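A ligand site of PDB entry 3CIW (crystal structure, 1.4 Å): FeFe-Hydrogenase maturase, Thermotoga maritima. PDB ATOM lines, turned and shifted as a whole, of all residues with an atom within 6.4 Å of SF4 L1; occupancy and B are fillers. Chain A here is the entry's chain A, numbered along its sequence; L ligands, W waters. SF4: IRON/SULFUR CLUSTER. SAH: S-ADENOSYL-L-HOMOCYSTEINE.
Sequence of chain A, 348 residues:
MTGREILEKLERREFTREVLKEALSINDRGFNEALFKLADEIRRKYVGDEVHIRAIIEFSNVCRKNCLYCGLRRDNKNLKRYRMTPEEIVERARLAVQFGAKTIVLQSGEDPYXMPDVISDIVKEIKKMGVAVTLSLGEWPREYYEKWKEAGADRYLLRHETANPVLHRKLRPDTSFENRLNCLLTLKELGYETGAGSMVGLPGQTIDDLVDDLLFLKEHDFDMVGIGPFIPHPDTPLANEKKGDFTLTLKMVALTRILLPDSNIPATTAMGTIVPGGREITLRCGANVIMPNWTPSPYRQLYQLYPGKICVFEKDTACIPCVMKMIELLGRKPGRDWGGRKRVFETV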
ATOM      1  N   VAL A  62       5.182  10.091   1.076  1.00  0.00           N
ATOM      2  CA  VAL A  62       6.074   9.200   1.827  1.00  0.00           C
ATOM      3  C   VAL A  62       5.262   8.510   2.909  1.00  0.00           C
ATOM      4  O   VAL A  62       4.484   9.148   3.603  1.00  0.00           O
ATOM      5  CB  VAL A  62       7.241   9.977   2.422  1.00  0.00           C
ATOM      6  CG1 VAL A  62       8.087   9.089   3.394  1.00  0.00           C
ATOM      7  CG2 VAL A  62       8.111  10.565   1.301  1.00  0.00           C
ATOM      8  N   CYS A  63       5.409   7.205   3.043  1.00  0.00           N
ATOM      9  CA  CYS A  63       4.732   6.494   4.105  1.00  0.00           C
ATOM     10  C   CYS A  63       5.566   5.392   4.715  1.00  0.00           C
ATOM     11  O   CYS A  63       6.234   4.651   3.997  1.00  0.00           O
ATOM     12  CB  CYS A  63       3.393   5.918   3.646  1.00  0.00           C
ATOM     13  SG  CYS A  63       2.374   5.450   5.092  1.00  0.00           S
ATOM     14  N   ARG A  64       5.502   5.285   6.048  1.00  0.00           N
ATOM     15  CA  ARG A  64       6.186   4.230   6.791  1.00  0.00           C
ATOM     16  C   ARG A  64       5.377   2.946   6.928  1.00  0.00           C
ATOM     17  O   ARG A  64       5.929   1.906   7.323  1.00  0.00           O
ATOM     18  CB  ARG A  64       6.533   4.723   8.182  1.00  0.00           C
ATOM     19  CG  ARG A  64       5.339   4.972   9.074  1.00  0.00           C
ATOM     20  CD  ARG A  64       5.681   5.570  10.402  1.00  0.00           C
ATOM     21  NE  ARG A  64       4.488   5.857  11.145  1.00  0.00           N
ATOM     22  CZ  ARG A  64       4.460   6.174  12.437  1.00  0.00           C
ATOM     23  NH1 ARG A  64       5.587   6.227  13.142  1.00  0.00           N
ATOM     24  NH2 ARG A  64       3.309   6.422  13.037  1.00  0.00           N
ATOM     25  N   LYS A  65       4.073   3.013   6.677  1.00  0.00           N
ATOM     26  CA  LYS A  65       3.213   1.851   6.802  1.00  0.00           C
ATOM     27  C   LYS A  65       3.073   1.118   5.479  1.00  0.00           C
ATOM     28  O   LYS A  65       3.481   1.610   4.433  1.00  0.00           O
ATOM     29  CB  LYS A  65       1.851   2.238   7.369  1.00  0.00           C
ATOM     30  CG  LYS A  65       1.828   2.413   8.886  1.00  0.00           C
ATOM     31  CD  LYS A  65       0.439   2.710   9.404  1.00  0.00           C
ATOM     32  CE  LYS A  65       0.357   2.597  10.907  1.00  0.00           C
ATOM     33  NZ  LYS A  65       1.339   3.416  11.672  1.00  0.00           N
ATOM     34  N   ASN A  66       2.463  -0.078   5.538  1.00  0.00           N
ATOM     35  CA  ASN A  66       2.441  -1.012   4.407  1.00  0.00           C
ATOM     36  C   ASN A  66       1.030  -1.572   4.156  1.00  0.00           C
ATOM     37  O   ASN A  66       0.871  -2.751   3.786  1.00  0.00           O
ATOM     38  CB  ASN A  66       3.453  -2.154   4.677  1.00  0.00           C
ATOM     39  CG  ASN A  66       4.087  -2.718   3.416  1.00  0.00           C
ATOM     40  OD1 ASN A  66       4.182  -2.049   2.384  1.00  0.00           O
ATOM     41  ND2 ASN A  66       4.614  -3.939   3.528  1.00  0.00           N
ATOM     42  N   CYS A  67       0.019  -0.727   4.323  1.00  0.00           N
ATOM     43  CA  CYS A  67      -1.372  -1.169   4.170  1.00  0.00           C
ATOM     44  C   CYS A  67      -1.537  -1.858   2.820  1.00  0.00           C
ATOM     45  O   CYS A  67      -1.039  -1.372   1.806  1.00  0.00           O
ATOM     46  CB  CYS A  67      -2.320   0.040   4.323  1.00  0.00           C
ATOM     47  SG  CYS A  67      -2.102   0.927   5.870  1.00  0.00           S
ATOM     48  N   LEU A  68      -2.196  -3.014   2.825  1.00  0.00           N
ATOM     49  CA  LEU A  68      -2.226  -3.849   1.624  1.00  0.00           C
ATOM     50  C   LEU A  68      -2.978  -3.242   0.470  1.00  0.00           C
ATOM     51  O   LEU A  68      -2.706  -3.579  -0.683  1.00  0.00           O
ATOM     52  CB  LEU A  68      -2.787  -5.234   1.941  1.00  0.00           C
ATOM     53  CG  LEU A  68      -1.775  -6.285   2.417  1.00  0.00           C
ATOM     54  CD1 LEU A  68      -1.056  -5.913   3.700  1.00  0.00           C
ATOM     55  CD2 LEU A  68      -2.493  -7.632   2.564  1.00  0.00           C
ATOM     56  N   TYR A  69      -3.921  -2.342   0.769  1.00  0.00           N
ATOM     57  CA  TYR A  69      -4.779  -1.735  -0.261  1.00  0.00           C
ATOM     58  C   TYR A  69      -4.196  -0.477  -0.892  1.00  0.00           C
ATOM     59  O   TYR A  69      -4.687  -0.049  -1.945  1.00  0.00           O
ATOM     60  CB  TYR A  69      -6.148  -1.384   0.327  1.00  0.00           C
ATOM     61  CG  TYR A  69      -6.084  -0.715   1.674  1.00  0.00           C
ATOM     62  CD1 TYR A  69      -5.796   0.648   1.799  1.00  0.00           C
ATOM     63  CD2 TYR A  69      -6.281  -1.441   2.837  1.00  0.00           C
ATOM     64  CE1 TYR A  69      -5.735   1.254   3.046  1.00  0.00           C
ATOM     65  CE2 TYR A  69      -6.214  -0.846   4.077  1.00  0.00           C
ATOM     66  CZ  TYR A  69      -5.949   0.497   4.189  1.00  0.00           C
ATOM     67  OH  TYR A  69      -5.855   1.078   5.428  1.00  0.00           O
ATOM     68  N   CYS A  70      -3.171   0.111  -0.271  1.00  0.00           N
ATOM     69  CA  CYS A  70      -2.794   1.487  -0.574  1.00  0.00           C
ATOM     70  C   CYS A  70      -1.589   1.613  -1.492  1.00  0.00           C
ATOM     71  O   CYS A  70      -0.537   1.031  -1.212  1.00  0.00           O
ATOM     72  CB  CYS A  70      -2.498   2.195   0.722  1.00  0.00           C
ATOM     73  SG  CYS A  70      -2.172   3.972   0.487  1.00  0.00           S
ATOM     74  N   GLY A  71      -1.711   2.408  -2.543  1.00  0.00           N
ATOM     75  CA  GLY A  71      -0.607   2.665  -3.442  1.00  0.00           C
ATOM     76  C   GLY A  71       0.587   3.365  -2.848  1.00  0.00           C
ATOM     77  O   GLY A  71       1.679   3.283  -3.409  1.00  0.00           O
ATOM     78  N   LEU A  72       0.425   4.027  -1.697  1.00  0.00           N
ATOM     79  CA  LEU A  72       1.551   4.675  -1.038  1.00  0.00           C
ATOM     80  C   LEU A  72       2.294   3.760  -0.076  1.00  0.00           C
ATOM     81  O   LEU A  72       3.241   4.174   0.540  1.00  0.00           O
ATOM     82  CB  LEU A  72       1.089   5.923  -0.260  1.00  0.00           C
ATOM     83  CG  LEU A  72       0.326   7.002  -1.029  1.00  0.00           C
ATOM     84  CD1 LEU A  72       0.287   8.281  -0.190  1.00  0.00           C
ATOM     85  CD2 LEU A  72       0.801   7.257  -2.412  1.00  0.00           C
ATOM     86  N   ARG A  73       1.851   2.511   0.047  1.00  0.00           N
ATOM     87  CA  ARG A  73       2.488   1.547   0.977  1.00  0.00           C
ATOM     88  C   ARG A  73       3.989   1.507   0.789  1.00  0.00           C
ATOM     89  O   ARG A  73       4.498   1.652  -0.328  1.00  0.00           O
ATOM     90  CB  ARG A  73       1.881   0.155   0.836  1.00  0.00           C
ATOM     91  CG  ARG A  73       2.171  -0.504  -0.497  1.00  0.00           C
ATOM     92  CD  ARG A  73       1.215  -1.670  -0.735  1.00  0.00           C
ATOM     93  NE  ARG A  73       1.198  -2.591   0.398  1.00  0.00           N
ATOM     94  CZ  ARG A  73       1.984  -3.659   0.543  1.00  0.00           C
ATOM     95  NH1 ARG A  73       2.854  -3.989  -0.386  1.00  0.00           N
ATOM     96  NH2 ARG A  73       1.857  -4.397   1.640  1.00  0.00           N
ATOM     97  N   ARG A  74       4.721   1.330   1.883  1.00  0.00           N
ATOM     98  CA  ARG A  74       6.171   1.509   1.812  1.00  0.00           C
ATOM     99  C   ARG A  74       6.855   0.557   0.844  1.00  0.00           C
ATOM    100  O   ARG A  74       7.873   0.926   0.260  1.00  0.00           O
ATOM    101  CB  ARG A  74       6.842   1.430   3.179  1.00  0.00           C
ATOM    102  CG  ARG A  74       6.757   0.109   3.859  1.00  0.00           C
ATOM    103  CD  ARG A  74       7.660   0.029   5.110  1.00  0.00           C
ATOM    104  NE  ARG A  74       7.532  -1.337   5.580  1.00  0.00           N
ATOM    105  CZ  ARG A  74       6.655  -1.765   6.490  1.00  0.00           C
ATOM    106  NH1 ARG A  74       5.860  -0.937   7.151  1.00  0.00           N
ATOM    107  NH2 ARG A  74       6.573  -3.046   6.760  1.00  0.00           N
ATOM    108  N   SER A 108      -1.377  13.354   4.172  1.00  0.00           N
ATOM    109  CA  SER A 108      -0.147  12.742   3.715  1.00  0.00           C
ATOM    110  C   SER A 108      -0.130  11.276   4.058  1.00  0.00           C
ATOM    111  O   SER A 108      -0.938  10.771   4.844  1.00  0.00           O
ATOM    112  CB  SER A 108       1.046  13.435   4.373  1.00  0.00           C
ATOM    113  OG  SER A 108       1.029  13.281   5.795  1.00  0.00           O
ATOM    114  N   GLY A 109       0.845  10.595   3.476  1.00  0.00           N
ATOM    115  CA  GLY A 109       1.271   9.313   4.052  1.00  0.00           C
ATOM    116  C   GLY A 109       1.794   9.556   5.448  1.00  0.00           C
ATOM    117  O   GLY A 109       2.029  10.705   5.850  1.00  0.00           O
ATOM    118  N   GLU A 110       2.031   8.484   6.202  1.00  0.00           N
ATOM    119  CA  GLU A 110       2.662   8.616   7.501  1.00  0.00           C
ATOM    120  C   GLU A 110       4.155   8.850   7.287  1.00  0.00           C
ATOM    121  O   GLU A 110       4.987   7.925   7.325  1.00  0.00           O
ATOM    122  CB  GLU A 110       2.406   7.385   8.359  1.00  0.00           C
ATOM    123  CG  GLU A 110       0.959   7.265   8.806  1.00  0.00           C
ATOM    124  CD  GLU A 110       0.761   6.278   9.946  1.00  0.00           C
ATOM    125  OE1 GLU A 110       1.776   5.798  10.483  1.00  0.00           O
ATOM    126  OE2 GLU A 110      -0.402   5.996  10.295  1.00  0.00           O
ATOM    127  N   GLY A 138      -2.642  10.175   9.643  1.00  0.00           N
ATOM    128  CA  GLY A 138      -2.529   8.814  10.160  1.00  0.00           C
ATOM    129  C   GLY A 138      -2.350   8.750  11.660  1.00  0.00           C
ATOM    130  O   GLY A 138      -2.771   9.643  12.405  1.00  0.00           O
ATOM    131  N   GLU A 161     -11.505   2.369   8.700  1.00  0.00           N
ATOM    132  CA  GLU A 161     -11.187   1.484   7.570  1.00  0.00           C
ATOM    133  C   GLU A 161     -12.086   0.259   7.527  1.00  0.00           C
ATOM    134  O   GLU A 161     -12.748  -0.004   6.518  1.00  0.00           O
ATOM    135  CB  GLU A 161      -9.701   1.073   7.536  1.00  0.00           C
ATOM    136  CG  GLU A 161      -8.701   2.223   7.666  1.00  0.00           C
ATOM    137  CD  GLU A 161      -8.789   3.286   6.587  1.00  0.00           C
ATOM    138  OE1 GLU A 161      -9.657   3.249   5.695  1.00  0.00           O
ATOM    139  OE2 GLU A 161      -7.935   4.200   6.672  1.00  0.00           O
ATOM    140  N   ARG A 172      -3.717  -4.095   7.436  1.00  0.00           N
ATOM    141  CA  ARG A 172      -2.914  -3.013   7.999  1.00  0.00           C
ATOM    142  C   ARG A 172      -1.925  -3.649   8.988  1.00  0.00           C
ATOM    143  O   ARG A 172      -2.080  -3.529  10.219  1.00  0.00           O
ATOM    144  CB  ARG A 172      -3.829  -1.980   8.637  1.00  0.00           C
ATOM    145  CG  ARG A 172      -4.964  -1.547   7.716  1.00  0.00           C
ATOM    146  CD  ARG A 172      -5.750  -0.313   8.181  1.00  0.00           C
ATOM    147  NE  ARG A 172      -4.843   0.820   8.188  1.00  0.00           N
ATOM    148  CZ  ARG A 172      -4.405   1.476   9.243  1.00  0.00           C
ATOM    149  NH1 ARG A 172      -4.871   1.231  10.456  1.00  0.00           N
ATOM    150  NH2 ARG A 172      -3.489   2.420   9.100  1.00  0.00           N
ATOM    151  N   ARG A 180      -6.278   1.932  16.094  1.00  0.00           N
ATOM    152  CA  ARG A 180      -7.035   2.913  15.311  1.00  0.00           C
ATOM    153  C   ARG A 180      -8.125   3.545  16.152  1.00  0.00           C
ATOM    154  O   ARG A 180      -8.278   4.783  16.152  1.00  0.00           O
ATOM    155  CB  ARG A 180      -7.630   2.231  14.084  1.00  0.00           C
ATOM    156  CG  ARG A 180      -8.043   3.166  12.954  1.00  0.00           C
ATOM    157  CD  ARG A 180      -6.839   3.691  12.223  1.00  0.00           C
ATOM    158  NE  ARG A 180      -7.189   4.386  10.989  1.00  0.00           N
ATOM    159  CZ  ARG A 180      -6.301   4.961  10.186  1.00  0.00           C
ATOM    160  NH1 ARG A 180      -5.010   4.932  10.466  1.00  0.00           N
ATOM    161  NH2 ARG A 180      -6.695   5.624   9.088  1.00  0.00           N
ATOM    162  N   TYR A 303       0.251  11.207  -5.972  1.00  0.00           N
ATOM    163  CA  TYR A 303      -0.465  10.827  -4.771  1.00  0.00           C
ATOM    164  C   TYR A 303      -1.541   9.855  -5.152  1.00  0.00           C
ATOM    165  O   TYR A 303      -2.693  10.212  -5.308  1.00  0.00           O
ATOM    166  CB  TYR A 303      -1.038  12.043  -4.081  1.00  0.00           C
ATOM    167  CG  TYR A 303      -1.469  11.782  -2.657  1.00  0.00           C
ATOM    168  CD1 TYR A 303      -0.553  11.789  -1.604  1.00  0.00           C
ATOM    169  CD2 TYR A 303      -2.802  11.523  -2.358  1.00  0.00           C
ATOM    170  CE1 TYR A 303      -0.958  11.569  -0.301  1.00  0.00           C
ATOM    171  CE2 TYR A 303      -3.204  11.310  -1.062  1.00  0.00           C
ATOM    172  CZ  TYR A 303      -2.287  11.323  -0.044  1.00  0.00           C
ATOM    173  OH  TYR A 303      -2.724  11.127   1.239  1.00  0.00           O
ATOM    174  N   LEU A 305      -3.242   6.850  -3.958  1.00  0.00           N
ATOM    175  CA  LEU A 305      -3.764   5.859  -2.995  1.00  0.00           C
ATOM    176  C   LEU A 305      -4.398   4.711  -3.799  1.00  0.00           C
ATOM    177  O   LEU A 305      -4.216   3.549  -3.496  1.00  0.00           O
ATOM    178  CB  LEU A 305      -4.795   6.510  -2.058  1.00  0.00           C
ATOM    179  CG  LEU A 305      -4.357   7.711  -1.218  1.00  0.00           C
ATOM    180  CD1 LEU A 305      -5.576   8.368  -0.548  1.00  0.00           C
ATOM    181  CD2 LEU A 305      -3.350   7.282  -0.178  1.00  0.00           C
HETATM  182 FE1  SF4 L   1      -1.729   3.108   5.035  1.00  0.00          FE
HETATM  183 FE2  SF4 L   1      -2.370   5.858   4.974  1.00  0.00          FE
HETATM  184 FE3  SF4 L   1       0.255   4.881   4.444  1.00  0.00          FE
HETATM  185 FE4  SF4 L   1      -1.675   4.406   2.657  1.00  0.00          FE
HETATM  186  S1  SF4 L   1      -0.892   6.436   3.213  1.00  0.00           S
HETATM  187  S2  SF4 L   1      -0.100   2.895   3.390  1.00  0.00           S
HETATM  188  S3  SF4 L   1      -3.535   4.129   3.997  1.00  0.00           S
HETATM  189  S4  SF4 L   1      -0.921   4.699   6.429  1.00  0.00           S
HETATM  190  N   SAH L   2      -2.114   7.978   5.785  1.00  0.00           N
HETATM  191  CA  SAH L   2      -3.376   8.567   6.293  1.00  0.00           C
HETATM  192  CB  SAH L   2      -4.051   9.446   5.243  1.00  0.00           C
HETATM  193  CG  SAH L   2      -3.955   9.012   3.793  1.00  0.00           C
HETATM  194  SD  SAH L   2      -4.883   7.519   3.388  1.00  0.00           S
HETATM  195  C   SAH L   2      -4.272   7.435   6.781  1.00  0.00           C
HETATM  196  O   SAH L   2      -3.978   6.256   6.471  1.00  0.00           O
HETATM  197  OXT SAH L   2      -5.270   7.709   7.467  1.00  0.00           O
HETATM  198  C5' SAH L   2      -6.577   8.210   3.348  1.00  0.00           C
HETATM  199  C4' SAH L   2      -7.685   7.193   3.039  1.00  0.00           C
HETATM  200  O4' SAH L   2      -7.650   6.695   1.703  1.00  0.00           O
HETATM  201  C3' SAH L   2      -7.635   5.923   3.891  1.00  0.00           C
HETATM  202  O3' SAH L   2      -8.207   6.170   5.147  1.00  0.00           O
HETATM  203  C2' SAH L   2      -8.385   4.882   3.051  1.00  0.00           C
HETATM  204  O2' SAH L   2      -9.734   4.695   3.450  1.00  0.00           O
HETATM  205  C1' SAH L   2      -8.351   5.488   1.617  1.00  0.00           C
HETATM  206  N9  SAH L   2      -7.737   4.573   0.666  1.00  0.00           N
HETATM  207  C8  SAH L   2      -6.444   4.110   0.674  1.00  0.00           C
HETATM  208  N7  SAH L   2      -6.269   3.221  -0.337  1.00  0.00           N
HETATM  209  C5  SAH L   2      -7.457   3.065  -0.977  1.00  0.00           C
HETATM  210  C6  SAH L   2      -7.857   2.333  -2.070  1.00  0.00           C
HETATM  211  N6  SAH L   2      -7.041   1.478  -2.703  1.00  0.00           N
HETATM  212  N1  SAH L   2      -9.153   2.427  -2.463  1.00  0.00           N
HETATM  213  C2  SAH L   2     -10.040   3.278  -1.862  1.00  0.00           C
HETATM  214  N3  SAH L   2      -9.637   4.040  -0.811  1.00  0.00           N
HETATM  215  C4  SAH L   2      -8.376   3.941  -0.367  1.00  0.00           C
HETATM  216  O   HOH W   1      -5.286   3.512   6.646  1.00  0.00           O
HETATM  217  O   HOH W   2      -2.709   5.618   9.041  1.00  0.00           O
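CB of Lys 65 touches S4 of SF4 L1 (3.8 Å).
Tyr 69 touches SF4 L1.
Arg 73 touches SF4 L1 (CA to S2, 3.8 Å).
CA of Gly 109 touches S1 of SF4 L1, 3.7 Å away.
CG of Glu 110 touches S4 of SF4 L1 (3.97 Å).
Hydrophobic or aromatic side chains that line SF4 L1: Tyr 69.
Along chain A the residues within 4 Å of SF4 L1 span positions 63 to 110.
The side-chain sulfur (SG) of Cys 63 lies close to the backbone NH (N) of Glu 110, at 3.2 Å.
O of Lys 65 sits at hydrogen-bond distance from N of Arg 74 (2.8 Å).
The side-chain sulfur (SG) of Cys 67 lies close to the side-chain hydroxyl (OH) of Tyr 69 (3.8 Å).
NZ of Lys 65 lies within salt-bridge range of OE1 of Glu 110 (2.7 Å).
OE1 of Glu 110 is in salt-bridge range of NE of Arg 64 (2.8 Å).
The backbone NH (N) of Leu 72 sits close to the side-chain sulfur (SG) of Cys 70 (3.4 Å).
The backbone carbonyl oxygen (O) of Cys 67 sits at hydrogen-bond distance from the guanidinium group (NE) of Arg 73 (2.9 Å).
The guanidinium group (NH2) of Arg 73 lies within hydrogen-bond range of the backbone carbonyl oxygen (O) of Asn 66 (2.9 Å).
Water W1 lies within hydrogen-bond range of OE2 of Glu 161 (2.7 Å), OH of Tyr 69 (2.8 Å), NE of Arg 172 (3.1 Å) and S3 of SF4 L1 (3.2 Å).
Water W2 lies within hydrogen-bond range of the side-chain carboxylate of Glu 110 (2.7 Å), the guanidinium group of Arg 180 (2.8 Å), the guanidinium group of Arg 172 (3.3 Å) and a sulfur (S4) of SF4 L1 (3.3 Å).
The side-chain sulfur (SG) of Cys 63 binds an iron atom (FE3) of SF4 L1 (2.3 Å).
S2 of SF4 L1 lies close to N of Cys 67.
The backbone carbonyl oxygen (O) of Tyr 69 lies within hydrogen-bond range of a nitrogen (N6) of SAH L2, at 2.9 Å.
The side-chain carboxylate of Glu 161 lies within hydrogen-bond range of an oxygen (O3') of SAH L2 (2.5 Å).
NH2 of Arg 180 lies within salt-bridge range of OXT of SAH L2, 3.0 Å away.
FE1 of SF4 L1 is bound by SG of Cys 67, 2.4 Å away.
O of Ser 108 sits close to N of SAH L2 (3.2 Å).
FE4 of SF4 L1 is bound by SG of Cys 70 (2.3 Å).
O of SAH L2 is bound to FE2 of SF4 L1, at 2.2 Å.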
